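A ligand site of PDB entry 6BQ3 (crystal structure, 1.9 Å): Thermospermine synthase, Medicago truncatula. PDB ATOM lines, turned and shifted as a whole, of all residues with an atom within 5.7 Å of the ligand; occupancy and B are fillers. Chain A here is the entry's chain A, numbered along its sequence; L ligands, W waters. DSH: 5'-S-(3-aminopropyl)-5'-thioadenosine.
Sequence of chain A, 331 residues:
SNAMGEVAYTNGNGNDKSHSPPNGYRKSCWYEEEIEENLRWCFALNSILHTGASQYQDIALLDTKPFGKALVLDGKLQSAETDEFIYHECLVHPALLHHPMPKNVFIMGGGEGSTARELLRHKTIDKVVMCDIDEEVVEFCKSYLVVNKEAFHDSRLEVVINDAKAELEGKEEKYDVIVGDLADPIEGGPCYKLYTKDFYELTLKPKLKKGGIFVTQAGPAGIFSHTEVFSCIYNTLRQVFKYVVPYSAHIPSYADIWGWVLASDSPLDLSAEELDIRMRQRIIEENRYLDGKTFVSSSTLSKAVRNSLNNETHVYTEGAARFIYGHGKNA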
ATOM      1  N   GLN A  57      21.209   6.084 -30.534  1.00  0.00           N
ATOM      2  CA  GLN A  57      21.979   5.637 -29.387  1.00  0.00           C
ATOM      3  C   GLN A  57      22.477   4.231 -29.562  1.00  0.00           C
ATOM      4  O   GLN A  57      22.013   3.478 -30.418  1.00  0.00           O
ATOM      5  CB  GLN A  57      21.088   5.694 -28.147  1.00  0.00           C
ATOM      6  CG  GLN A  57      19.872   4.776 -28.245  1.00  0.00           C
ATOM      7  CD  GLN A  57      18.606   5.373 -27.658  1.00  0.00           C
ATOM      8  OE1 GLN A  57      18.652   6.063 -26.645  1.00  0.00           O
ATOM      9  NE2 GLN A  57      17.476   5.085 -28.288  1.00  0.00           N
ATOM     10  N   LEU A  73      21.479   1.855 -22.661  1.00  0.00           N
ATOM     11  CA  LEU A  73      21.357   2.803 -23.783  1.00  0.00           C
ATOM     12  C   LEU A  73      22.426   3.842 -23.662  1.00  0.00           C
ATOM     13  O   LEU A  73      22.543   4.502 -22.614  1.00  0.00           O
ATOM     14  CB  LEU A  73      19.954   3.473 -23.843  1.00  0.00           C
ATOM     15  CG  LEU A  73      18.745   2.512 -23.949  1.00  0.00           C
ATOM     16  CD1 LEU A  73      17.409   3.210 -24.112  1.00  0.00           C
ATOM     17  CD2 LEU A  73      18.931   1.506 -25.072  1.00  0.00           C
ATOM     18  N   GLN A  78      19.182   1.392 -18.227  1.00  0.00           N
ATOM     19  CA  GLN A  78      17.885   2.073 -18.214  1.00  0.00           C
ATOM     20  C   GLN A  78      16.739   1.183 -17.704  1.00  0.00           C
ATOM     21  O   GLN A  78      15.757   1.682 -17.291  1.00  0.00           O
ATOM     22  CB  GLN A  78      17.572   2.678 -19.593  1.00  0.00           C
ATOM     23  CG  GLN A  78      18.460   3.859 -19.987  1.00  0.00           C
ATOM     24  CD  GLN A  78      18.221   5.117 -19.143  1.00  0.00           C
ATOM     25  OE1 GLN A  78      17.441   5.116 -18.183  1.00  0.00           O
ATOM     26  NE2 GLN A  78      18.966   6.176 -19.430  1.00  0.00           N
ATOM     27  N   TYR A  87      10.457   1.098 -10.703  1.00  0.00           N
ATOM     28  CA  TYR A  87      10.446   2.264 -11.557  1.00  0.00           C
ATOM     29  C   TYR A  87       9.092   2.441 -12.241  1.00  0.00           C
ATOM     30  O   TYR A  87       8.535   3.539 -12.257  1.00  0.00           O
ATOM     31  CB  TYR A  87      11.594   2.192 -12.568  1.00  0.00           C
ATOM     32  CG  TYR A  87      11.606   3.328 -13.573  1.00  0.00           C
ATOM     33  CD1 TYR A  87      12.280   4.516 -13.317  1.00  0.00           C
ATOM     34  CD2 TYR A  87      10.893   3.223 -14.759  1.00  0.00           C
ATOM     35  CE1 TYR A  87      12.255   5.575 -14.224  1.00  0.00           C
ATOM     36  CE2 TYR A  87      10.838   4.289 -15.665  1.00  0.00           C
ATOM     37  CZ  TYR A  87      11.552   5.457 -15.405  1.00  0.00           C
ATOM     38  OH  TYR A  87      11.571   6.493 -16.297  1.00  0.00           O
ATOM     39  N   MET A 108       5.786   9.591 -23.696  1.00  0.00           N
ATOM     40  CA  MET A 108       6.953  10.131 -24.387  1.00  0.00           C
ATOM     41  C   MET A 108       8.115   9.213 -24.076  1.00  0.00           C
ATOM     42  O   MET A 108       8.560   9.173 -22.923  1.00  0.00           O
ATOM     43  CB  MET A 108       7.217  11.540 -23.877  1.00  0.00           C
ATOM     44  CG  MET A 108       5.986  12.421 -23.850  1.00  0.00           C
ATOM     45  SD  MET A 108       6.401  14.175 -23.633  1.00  0.00           S
ATOM     46  CE  MET A 108       7.007  14.142 -21.939  1.00  0.00           C
ATOM     47  N   GLY A 109       8.594   8.468 -25.084  1.00  0.00           N
ATOM     48  CA  GLY A 109       9.460   7.301 -24.874  1.00  0.00           C
ATOM     49  C   GLY A 109       8.652   5.988 -24.791  1.00  0.00           C
ATOM     50  O   GLY A 109       7.754   5.720 -25.605  1.00  0.00           O
ATOM     51  N   GLY A 110       8.965   5.172 -23.802  1.00  0.00           N
ATOM     52  CA  GLY A 110       8.244   3.923 -23.560  1.00  0.00           C
ATOM     53  C   GLY A 110       8.685   2.734 -24.379  1.00  0.00           C
ATOM     54  O   GLY A 110       8.093   1.653 -24.254  1.00  0.00           O
ATOM     55  N   GLY A 111       9.722   2.891 -25.225  1.00  0.00           N
ATOM     56  CA  GLY A 111      10.149   1.824 -26.130  1.00  0.00           C
ATOM     57  C   GLY A 111      10.438   0.499 -25.456  1.00  0.00           C
ATOM     58  O   GLY A 111      10.197  -0.563 -26.014  1.00  0.00           O
ATOM     59  N   GLU A 112      10.939   0.565 -24.223  1.00  0.00           N
ATOM     60  CA  GLU A 112      11.201  -0.604 -23.401  1.00  0.00           C
ATOM     61  C   GLU A 112       9.933  -1.414 -23.063  1.00  0.00           C
ATOM     62  O   GLU A 112      10.009  -2.635 -22.791  1.00  0.00           O
ATOM     63  CB  GLU A 112      11.996  -0.161 -22.156  1.00  0.00           C
ATOM     64  CG  GLU A 112      12.334  -1.232 -21.167  1.00  0.00           C
ATOM     65  CD  GLU A 112      11.312  -1.353 -20.044  1.00  0.00           C
ATOM     66  OE1 GLU A 112      11.582  -2.106 -19.064  1.00  0.00           O
ATOM     67  OE2 GLU A 112      10.235  -0.674 -20.118  1.00  0.00           O
ATOM     68  N   CYS A 131       4.981   6.593 -27.873  1.00  0.00           N
ATOM     69  CA  CYS A 131       5.684   7.381 -28.853  1.00  0.00           C
ATOM     70  C   CYS A 131       7.197   7.406 -28.548  1.00  0.00           C
ATOM     71  O   CYS A 131       7.643   8.239 -27.760  1.00  0.00           O
ATOM     72  CB  CYS A 131       5.116   8.795 -28.929  1.00  0.00           C
ATOM     73  SG  CYS A 131       5.879   9.708 -30.296  1.00  0.00           S
ATOM     74  N   ASP A 132       7.958   6.509 -29.172  1.00  0.00           N
ATOM     75  CA  ASP A 132       9.417   6.491 -28.982  1.00  0.00           C
ATOM     76  C   ASP A 132      10.117   6.900 -30.277  1.00  0.00           C
ATOM     77  O   ASP A 132       9.657   6.548 -31.358  1.00  0.00           O
ATOM     78  CB  ASP A 132       9.877   5.110 -28.544  1.00  0.00           C
ATOM     79  CG  ASP A 132      11.230   5.121 -27.867  1.00  0.00           C
ATOM     80  OD1 ASP A 132      12.235   5.465 -28.540  1.00  0.00           O
ATOM     81  OD2 ASP A 132      11.280   4.778 -26.662  1.00  0.00           O
ATOM     82  N   ILE A 133      11.233   7.606 -30.162  1.00  0.00           N
ATOM     83  CA  ILE A 133      11.971   8.072 -31.334  1.00  0.00           C
ATOM     84  C   ILE A 133      12.755   6.944 -32.039  1.00  0.00           C
ATOM     85  O   ILE A 133      13.124   7.073 -33.214  1.00  0.00           O
ATOM     86  CB  ILE A 133      12.852   9.272 -30.913  1.00  0.00           C
ATOM     87  CG1 ILE A 133      13.216  10.137 -32.117  1.00  0.00           C
ATOM     88  CG2 ILE A 133      14.085   8.823 -30.138  1.00  0.00           C
ATOM     89  CD1 ILE A 133      13.903  11.420 -31.715  1.00  0.00           C
ATOM     90  N   ASP A 134      12.974   5.823 -31.334  1.00  0.00           N
ATOM     91  CA  ASP A 134      13.896   4.772 -31.779  1.00  0.00           C
ATOM     92  C   ASP A 134      13.167   3.430 -31.993  1.00  0.00           C
ATOM     93  O   ASP A 134      13.002   2.618 -31.084  1.00  0.00           O
ATOM     94  CB  ASP A 134      15.077   4.639 -30.795  1.00  0.00           C
ATOM     95  CG  ASP A 134      16.297   3.973 -31.429  1.00  0.00           C
ATOM     96  OD1 ASP A 134      16.139   3.239 -32.419  1.00  0.00           O
ATOM     97  OD2 ASP A 134      17.425   4.206 -30.943  1.00  0.00           O
ATOM     98  N   VAL A 137      14.971   0.313 -30.604  1.00  0.00           N
ATOM     99  CA  VAL A 137      14.768   0.027 -29.176  1.00  0.00           C
ATOM    100  C   VAL A 137      13.492  -0.784 -29.005  1.00  0.00           C
ATOM    101  O   VAL A 137      13.466  -1.789 -28.298  1.00  0.00           O
ATOM    102  CB  VAL A 137      14.621   1.312 -28.307  1.00  0.00           C
ATOM    103  CG1 VAL A 137      14.143   0.985 -26.886  1.00  0.00           C
ATOM    104  CG2 VAL A 137      15.915   2.088 -28.233  1.00  0.00           C
ATOM    105  N   ASN A 162       8.349   8.202 -33.505  1.00  0.00           N
ATOM    106  CA  ASN A 162       8.571   9.651 -33.688  1.00  0.00           C
ATOM    107  C   ASN A 162       9.225  10.276 -32.445  1.00  0.00           C
ATOM    108  O   ASN A 162       9.164   9.717 -31.305  1.00  0.00           O
ATOM    109  CB  ASN A 162       7.229  10.375 -33.942  1.00  0.00           C
ATOM    110  CG  ASN A 162       7.357  11.670 -34.774  1.00  0.00           C
ATOM    111  OD1 ASN A 162       8.450  12.093 -35.147  1.00  0.00           O
ATOM    112  ND2 ASN A 162       6.216  12.282 -35.090  1.00  0.00           N
ATOM    113  N   ASP A 163       9.784  11.453 -32.663  1.00  0.00           N
ATOM    114  CA  ASP A 163      10.072  12.387 -31.573  1.00  0.00           C
ATOM    115  C   ASP A 163       8.736  12.825 -30.951  1.00  0.00           C
ATOM    116  O   ASP A 163       7.909  13.349 -31.631  1.00  0.00           O
ATOM    117  CB  ASP A 163      10.881  13.594 -32.107  1.00  0.00           C
ATOM    118  CG  ASP A 163      10.865  14.780 -31.178  1.00  0.00           C
ATOM    119  OD1 ASP A 163      11.192  14.625 -30.001  1.00  0.00           O
ATOM    120  OD2 ASP A 163      10.435  15.864 -31.634  1.00  0.00           O
ATOM    121  N   ALA A 164       8.568  12.597 -29.645  1.00  0.00           N
ATOM    122  CA  ALA A 164       7.304  12.879 -28.961  1.00  0.00           C
ATOM    123  C   ALA A 164       6.899  14.344 -29.045  1.00  0.00           C
ATOM    124  O   ALA A 164       5.719  14.642 -29.027  1.00  0.00           O
ATOM    125  CB  ALA A 164       7.333  12.438 -27.516  1.00  0.00           C
ATOM    126  N   LYS A 165       7.871  15.249 -29.067  1.00  0.00           N
ATOM    127  CA  LYS A 165       7.572  16.677 -29.192  1.00  0.00           C
ATOM    128  C   LYS A 165       6.919  16.968 -30.570  1.00  0.00           C
ATOM    129  O   LYS A 165       5.918  17.678 -30.634  1.00  0.00           O
ATOM    130  CB  LYS A 165       8.849  17.505 -29.020  1.00  0.00           C
ATOM    131  CG  LYS A 165       8.711  18.965 -29.441  1.00  0.00           C
ATOM    132  CD  LYS A 165       9.833  19.825 -28.828  1.00  0.00           C
ATOM    133  CE  LYS A 165       9.946  21.227 -29.418  1.00  0.00           C
ATOM    134  NZ  LYS A 165       8.608  21.877 -29.640  1.00  0.00           N
ATOM    135  N   ASP A 181       8.685   9.320 -20.059  1.00  0.00           N
ATOM    136  CA  ASP A 181       9.501   8.152 -19.747  1.00  0.00           C
ATOM    137  C   ASP A 181      10.716   8.326 -20.653  1.00  0.00           C
ATOM    138  O   ASP A 181      11.164   7.399 -21.333  1.00  0.00           O
ATOM    139  CB  ASP A 181       8.713   6.861 -20.063  1.00  0.00           C
ATOM    140  CG  ASP A 181       9.402   5.574 -19.574  1.00  0.00           C
ATOM    141  OD1 ASP A 181      10.362   5.630 -18.777  1.00  0.00           O
ATOM    142  OD2 ASP A 181       8.956   4.487 -19.990  1.00  0.00           O
ATOM    143  N   LEU A 182      11.259   9.547 -20.593  1.00  0.00           N
ATOM    144  CA  LEU A 182      12.476   9.922 -21.334  1.00  0.00           C
ATOM    145  C   LEU A 182      13.743   9.772 -20.488  1.00  0.00           C
ATOM    146  O   LEU A 182      13.687   9.559 -19.272  1.00  0.00           O
ATOM    147  CB  LEU A 182      12.351  11.360 -21.794  1.00  0.00           C
ATOM    148  CG  LEU A 182      11.148  11.670 -22.662  1.00  0.00           C
ATOM    149  CD1 LEU A 182      10.925  13.180 -22.727  1.00  0.00           C
ATOM    150  CD2 LEU A 182      11.306  11.067 -24.063  1.00  0.00           C
ATOM    151  N   ALA A 183      14.891   9.871 -21.146  1.00  0.00           N
ATOM    152  CA  ALA A 183      16.182   9.979 -20.435  1.00  0.00           C
ATOM    153  C   ALA A 183      16.280  11.366 -19.828  1.00  0.00           C
ATOM    154  O   ALA A 183      15.620  12.271 -20.281  1.00  0.00           O
ATOM    155  CB  ALA A 183      17.357   9.710 -21.363  1.00  0.00           C
ATOM    156  N   ASP A 184      17.125  11.546 -18.805  1.00  0.00           N
ATOM    157  CA  ASP A 184      17.223  12.847 -18.113  1.00  0.00           C
ATOM    158  C   ASP A 184      17.543  13.983 -19.085  1.00  0.00           C
ATOM    159  O   ASP A 184      18.102  13.736 -20.151  1.00  0.00           O
ATOM    160  CB  ASP A 184      18.333  12.812 -17.060  1.00  0.00           C
ATOM    161  CG  ASP A 184      18.043  11.847 -15.916  1.00  0.00           C
ATOM    162  OD1 ASP A 184      16.902  11.344 -15.793  1.00  0.00           O
ATOM    163  OD2 ASP A 184      18.958  11.576 -15.168  1.00  0.00           O
ATOM    164  N   PRO A 190      18.613  14.142 -27.347  1.00  0.00           N
ATOM    165  CA  PRO A 190      17.288  14.205 -27.971  1.00  0.00           C
ATOM    166  C   PRO A 190      16.128  14.373 -26.965  1.00  0.00           C
ATOM    167  O   PRO A 190      14.957  14.419 -27.399  1.00  0.00           O
ATOM    168  CB  PRO A 190      17.188  12.831 -28.650  1.00  0.00           C
ATOM    169  CG  PRO A 190      17.931  11.914 -27.704  1.00  0.00           C
ATOM    170  CD  PRO A 190      18.988  12.757 -27.018  1.00  0.00           C
ATOM    171  N   CYS A 191      16.437  14.434 -25.656  1.00  0.00           N
ATOM    172  CA  CYS A 191      15.409  14.525 -24.600  1.00  0.00           C
ATOM    173  C   CYS A 191      15.307  15.890 -23.958  1.00  0.00           C
ATOM    174  O   CYS A 191      14.241  16.220 -23.422  1.00  0.00           O
ATOM    175  CB  CYS A 191      15.722  13.517 -23.486  1.00  0.00           C
ATOM    176  SG  CYS A 191      15.912  11.815 -24.053  1.00  0.00           S
ATOM    177  N   LYS A 193      14.921  19.018 -24.820  1.00  0.00           N
ATOM    178  CA  LYS A 193      13.787  19.853 -25.323  1.00  0.00           C
ATOM    179  C   LYS A 193      12.486  19.592 -24.528  1.00  0.00           C
ATOM    180  O   LYS A 193      11.706  20.518 -24.234  1.00  0.00           O
ATOM    181  CB  LYS A 193      13.456  19.473 -26.772  1.00  0.00           C
ATOM    182  CG  LYS A 193      14.502  19.781 -27.836  1.00  0.00           C
ATOM    183  CD  LYS A 193      14.682  18.639 -28.858  1.00  0.00           C
ATOM    184  CE  LYS A 193      13.413  18.099 -29.517  1.00  0.00           C
ATOM    185  NZ  LYS A 193      12.853  19.112 -30.448  1.00  0.00           N
ATOM    186  N   LEU A 194      12.272  18.319 -24.174  1.00  0.00           N
ATOM    187  CA  LEU A 194      10.991  17.836 -23.649  1.00  0.00           C
ATOM    188  C   LEU A 194      10.867  18.043 -22.131  1.00  0.00           C
ATOM    189  O   LEU A 194       9.915  17.532 -21.499  1.00  0.00           O
ATOM    190  CB  LEU A 194      10.783  16.365 -24.027  1.00  0.00           C
ATOM    191  CG  LEU A 194      10.393  16.073 -25.488  1.00  0.00           C
ATOM    192  CD1 LEU A 194      11.410  16.562 -26.486  1.00  0.00           C
ATOM    193  CD2 LEU A 194      10.157  14.592 -25.698  1.00  0.00           C
ATOM    194  N   GLN A 217       9.310  11.017 -15.331  1.00  0.00           N
ATOM    195  CA  GLN A 217      10.549  10.613 -14.658  1.00  0.00           C
ATOM    196  C   GLN A 217      11.422  11.878 -14.504  1.00  0.00           C
ATOM    197  O   GLN A 217      11.352  12.841 -15.322  1.00  0.00           O
ATOM    198  CB  GLN A 217      11.248   9.468 -15.401  1.00  0.00           C
ATOM    199  CG  GLN A 217      12.197   9.837 -16.562  1.00  0.00           C
ATOM    200  CD  GLN A 217      13.628  10.217 -16.065  1.00  0.00           C
ATOM    201  OE1 GLN A 217      14.223   9.471 -15.334  1.00  0.00           O
ATOM    202  NE2 GLN A 217      14.123  11.365 -16.435  1.00  0.00           N
ATOM    203  N   TYR A 254      19.832   1.440 -10.570  1.00  0.00           N
ATOM    204  CA  TYR A 254      20.168   2.814 -10.899  1.00  0.00           C
ATOM    205  C   TYR A 254      21.171   3.368  -9.902  1.00  0.00           C
ATOM    206  O   TYR A 254      21.622   4.490 -10.111  1.00  0.00           O
ATOM    207  CB  TYR A 254      18.917   3.711 -10.906  1.00  0.00           C
ATOM    208  CG  TYR A 254      17.985   3.590 -12.083  1.00  0.00           C
ATOM    209  CD1 TYR A 254      18.084   2.560 -13.041  1.00  0.00           C
ATOM    210  CD2 TYR A 254      16.969   4.526 -12.250  1.00  0.00           C
ATOM    211  CE1 TYR A 254      17.197   2.485 -14.099  1.00  0.00           C
ATOM    212  CE2 TYR A 254      16.095   4.479 -13.320  1.00  0.00           C
ATOM    213  CZ  TYR A 254      16.209   3.464 -14.249  1.00  0.00           C
ATOM    214  OH  TYR A 254      15.305   3.414 -15.310  1.00  0.00           O
ATOM    215  N   TRP A 258      15.559   7.420  -7.071  1.00  0.00           N
ATOM    216  CA  TRP A 258      15.101   8.057  -8.300  1.00  0.00           C
ATOM    217  C   TRP A 258      13.839   8.853  -8.039  1.00  0.00           C
ATOM    218  O   TRP A 258      13.039   8.509  -7.171  1.00  0.00           O
ATOM    219  CB  TRP A 258      14.828   7.015  -9.366  1.00  0.00           C
ATOM    220  CG  TRP A 258      15.111   7.473 -10.724  1.00  0.00           C
ATOM    221  CD1 TRP A 258      14.211   7.791 -11.694  1.00  0.00           C
ATOM    222  CD2 TRP A 258      16.392   7.708 -11.260  1.00  0.00           C
ATOM    223  NE1 TRP A 258      14.861   8.154 -12.828  1.00  0.00           N
ATOM    224  CE2 TRP A 258      16.210   8.112 -12.594  1.00  0.00           C
ATOM    225  CE3 TRP A 258      17.696   7.583 -10.744  1.00  0.00           C
ATOM    226  CZ2 TRP A 258      17.276   8.416 -13.430  1.00  0.00           C
ATOM    227  CZ3 TRP A 258      18.762   7.856 -11.585  1.00  0.00           C
ATOM    228  CH2 TRP A 258      18.543   8.290 -12.923  1.00  0.00           C
HETATM  229  N   DSH L   1      14.661   6.332 -16.984  1.00  0.00           N
HETATM  230  N1  DSH L   1      10.863  11.345 -28.200  1.00  0.00           N
HETATM  231  C2  DSH L   1      10.329  10.046 -27.922  1.00  0.00           C
HETATM  232  N3  DSH L   1      11.198   9.057 -27.295  1.00  0.00           N
HETATM  233  C4  DSH L   1      12.610   9.407 -26.945  1.00  0.00           C
HETATM  234  C5  DSH L   1      13.111  10.642 -27.210  1.00  0.00           C
HETATM  235  C6  DSH L   1      12.209  11.693 -27.880  1.00  0.00           C
HETATM  236  N6  DSH L   1      12.683  13.020 -28.188  1.00  0.00           N
HETATM  237  N7  DSH L   1      14.381  10.675 -26.799  1.00  0.00           N
HETATM  238  C8  DSH L   1      14.674   9.459 -26.272  1.00  0.00           C
HETATM  239  N9  DSH L   1      13.589   8.671 -26.366  1.00  0.00           N
HETATM  240  CA  DSH L   1      14.221   5.459 -18.078  1.00  0.00           C
HETATM  241  CB  DSH L   1      14.341   6.218 -19.425  1.00  0.00           C
HETATM  242  SD  DSH L   1      15.501   5.510 -21.887  1.00  0.00           S
HETATM  243  CG  DSH L   1      14.230   5.221 -20.616  1.00  0.00           C
HETATM  244  C1' DSH L   1      13.410   7.397 -25.950  1.00  0.00           C
HETATM  245  C2' DSH L   1      14.630   6.401 -26.105  1.00  0.00           C
HETATM  246  O2' DSH L   1      14.685   5.814 -27.501  1.00  0.00           O
HETATM  247  C3' DSH L   1      14.442   5.543 -25.195  1.00  0.00           C
HETATM  248  O3' DSH L   1      13.484   4.463 -25.520  1.00  0.00           O
HETATM  249  C4' DSH L   1      13.790   6.385 -23.923  1.00  0.00           C
HETATM  250  O4' DSH L   1      13.148   7.393 -24.454  1.00  0.00           O
HETATM  251  C5' DSH L   1      14.891   6.855 -22.992  1.00  0.00           C
HETATM  252  O   HOH W   1      12.365   2.769 -23.271  1.00  0.00           O
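An oxygen (O3') of the ligand lies within hydrogen-bond range of the side-chain carboxylate (OD2) of Asp 132 (2.5 Å).
O of Pro 190 sits at hydrogen-bond distance from N6 of the ligand.
A nitrogen (N6) of the ligand lies within hydrogen-bond range of the side-chain carboxylate of Asp 163 (2.8 Å).
N of Ala 164 lies within hydrogen-bond range of N1 of the ligand (3.0 Å).
O2' of the ligand sits at hydrogen-bond distance from NE2 of Gln 57.
OH of Tyr 87 is in hydrogen-bond range of N of the ligand (3.2 Å).
N of Ile 133 lies within hydrogen-bond range of N3 of the ligand (3.2 Å).
The side-chain amide oxygen (OE1) of Gln 78 lies close to a nitrogen (N) of the ligand (3.3 Å).
A nitrogen (N7) of the ligand lies within hydrogen-bond range of the side-chain sulfur (SG) of Cys 191.
The side-chain hydroxyl of Tyr 254 lies within hydrogen-bond range of a nitrogen (N) of the ligand (3.4 Å).
N3 of the ligand sits close to N of Gly 109, 3.5 Å away.
O of Asp 132 sits at hydrogen-bond distance from N of Asn 162, at 3.0 Å.
The backbone NH (N) of Gly 111 lies within hydrogen-bond range of the side-chain carboxylate (OD2) of Asp 132 (2.8 Å).
The side-chain carboxylate (OD2) of Asp 134 sits at hydrogen-bond distance from the side-chain amide nitrogen (NE2) of Gln 57 (2.8 Å).
The side-chain hydroxyl (OH) of Tyr 87 sits at hydrogen-bond distance from the side-chain carboxylate (OD1) of Asp 181, 2.9 Å away.
The backbone NH of Gly 109 lies within hydrogen-bond range of the backbone carbonyl oxygen of Cys 131, 2.8 Å away.
The side-chain sulfur (SG) of Cys 131 sits at hydrogen-bond distance from the backbone carbonyl oxygen (O) of Asn 162, 3.4 Å away.
The side-chain sulfur (SG) of Cys 191 lies within hydrogen-bond range of the backbone NH (N) of Ala 183, at 3.6 Å.
OE1 of Gln 217 sits at hydrogen-bond distance from NE1 of Trp 258, 2.9 Å away.
Residues that only touch the ligand: Leu 73 (3.7 Å), Cys 131 (3.2 Å), Asp 134 (3.5 Å), Val 137 (3.8 Å), Asn 162 (3.6 Å), Asp 181 (3.7 Å), Leu 182 (3.4 Å), Ala 183 (3.5 Å), Leu 194 (3.9 Å) and Gln 217 (3.6 Å).
Hydrophobic or aromatic side chains within 4 Å of the ligand: Leu 73, Tyr 87, Ile 133, Val 137, Ala 164, Leu 182, Pro 190 and Leu 194.
Of the 29 residues printed, 21 come within 4 Å of the ligand.
The nearest printed residue that does not touch the ligand is Gly 111 (4.1 Å).
Water W1 lies within hydrogen-bond range of N of Glu 112, O3' of the ligand and N of Gly 111.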
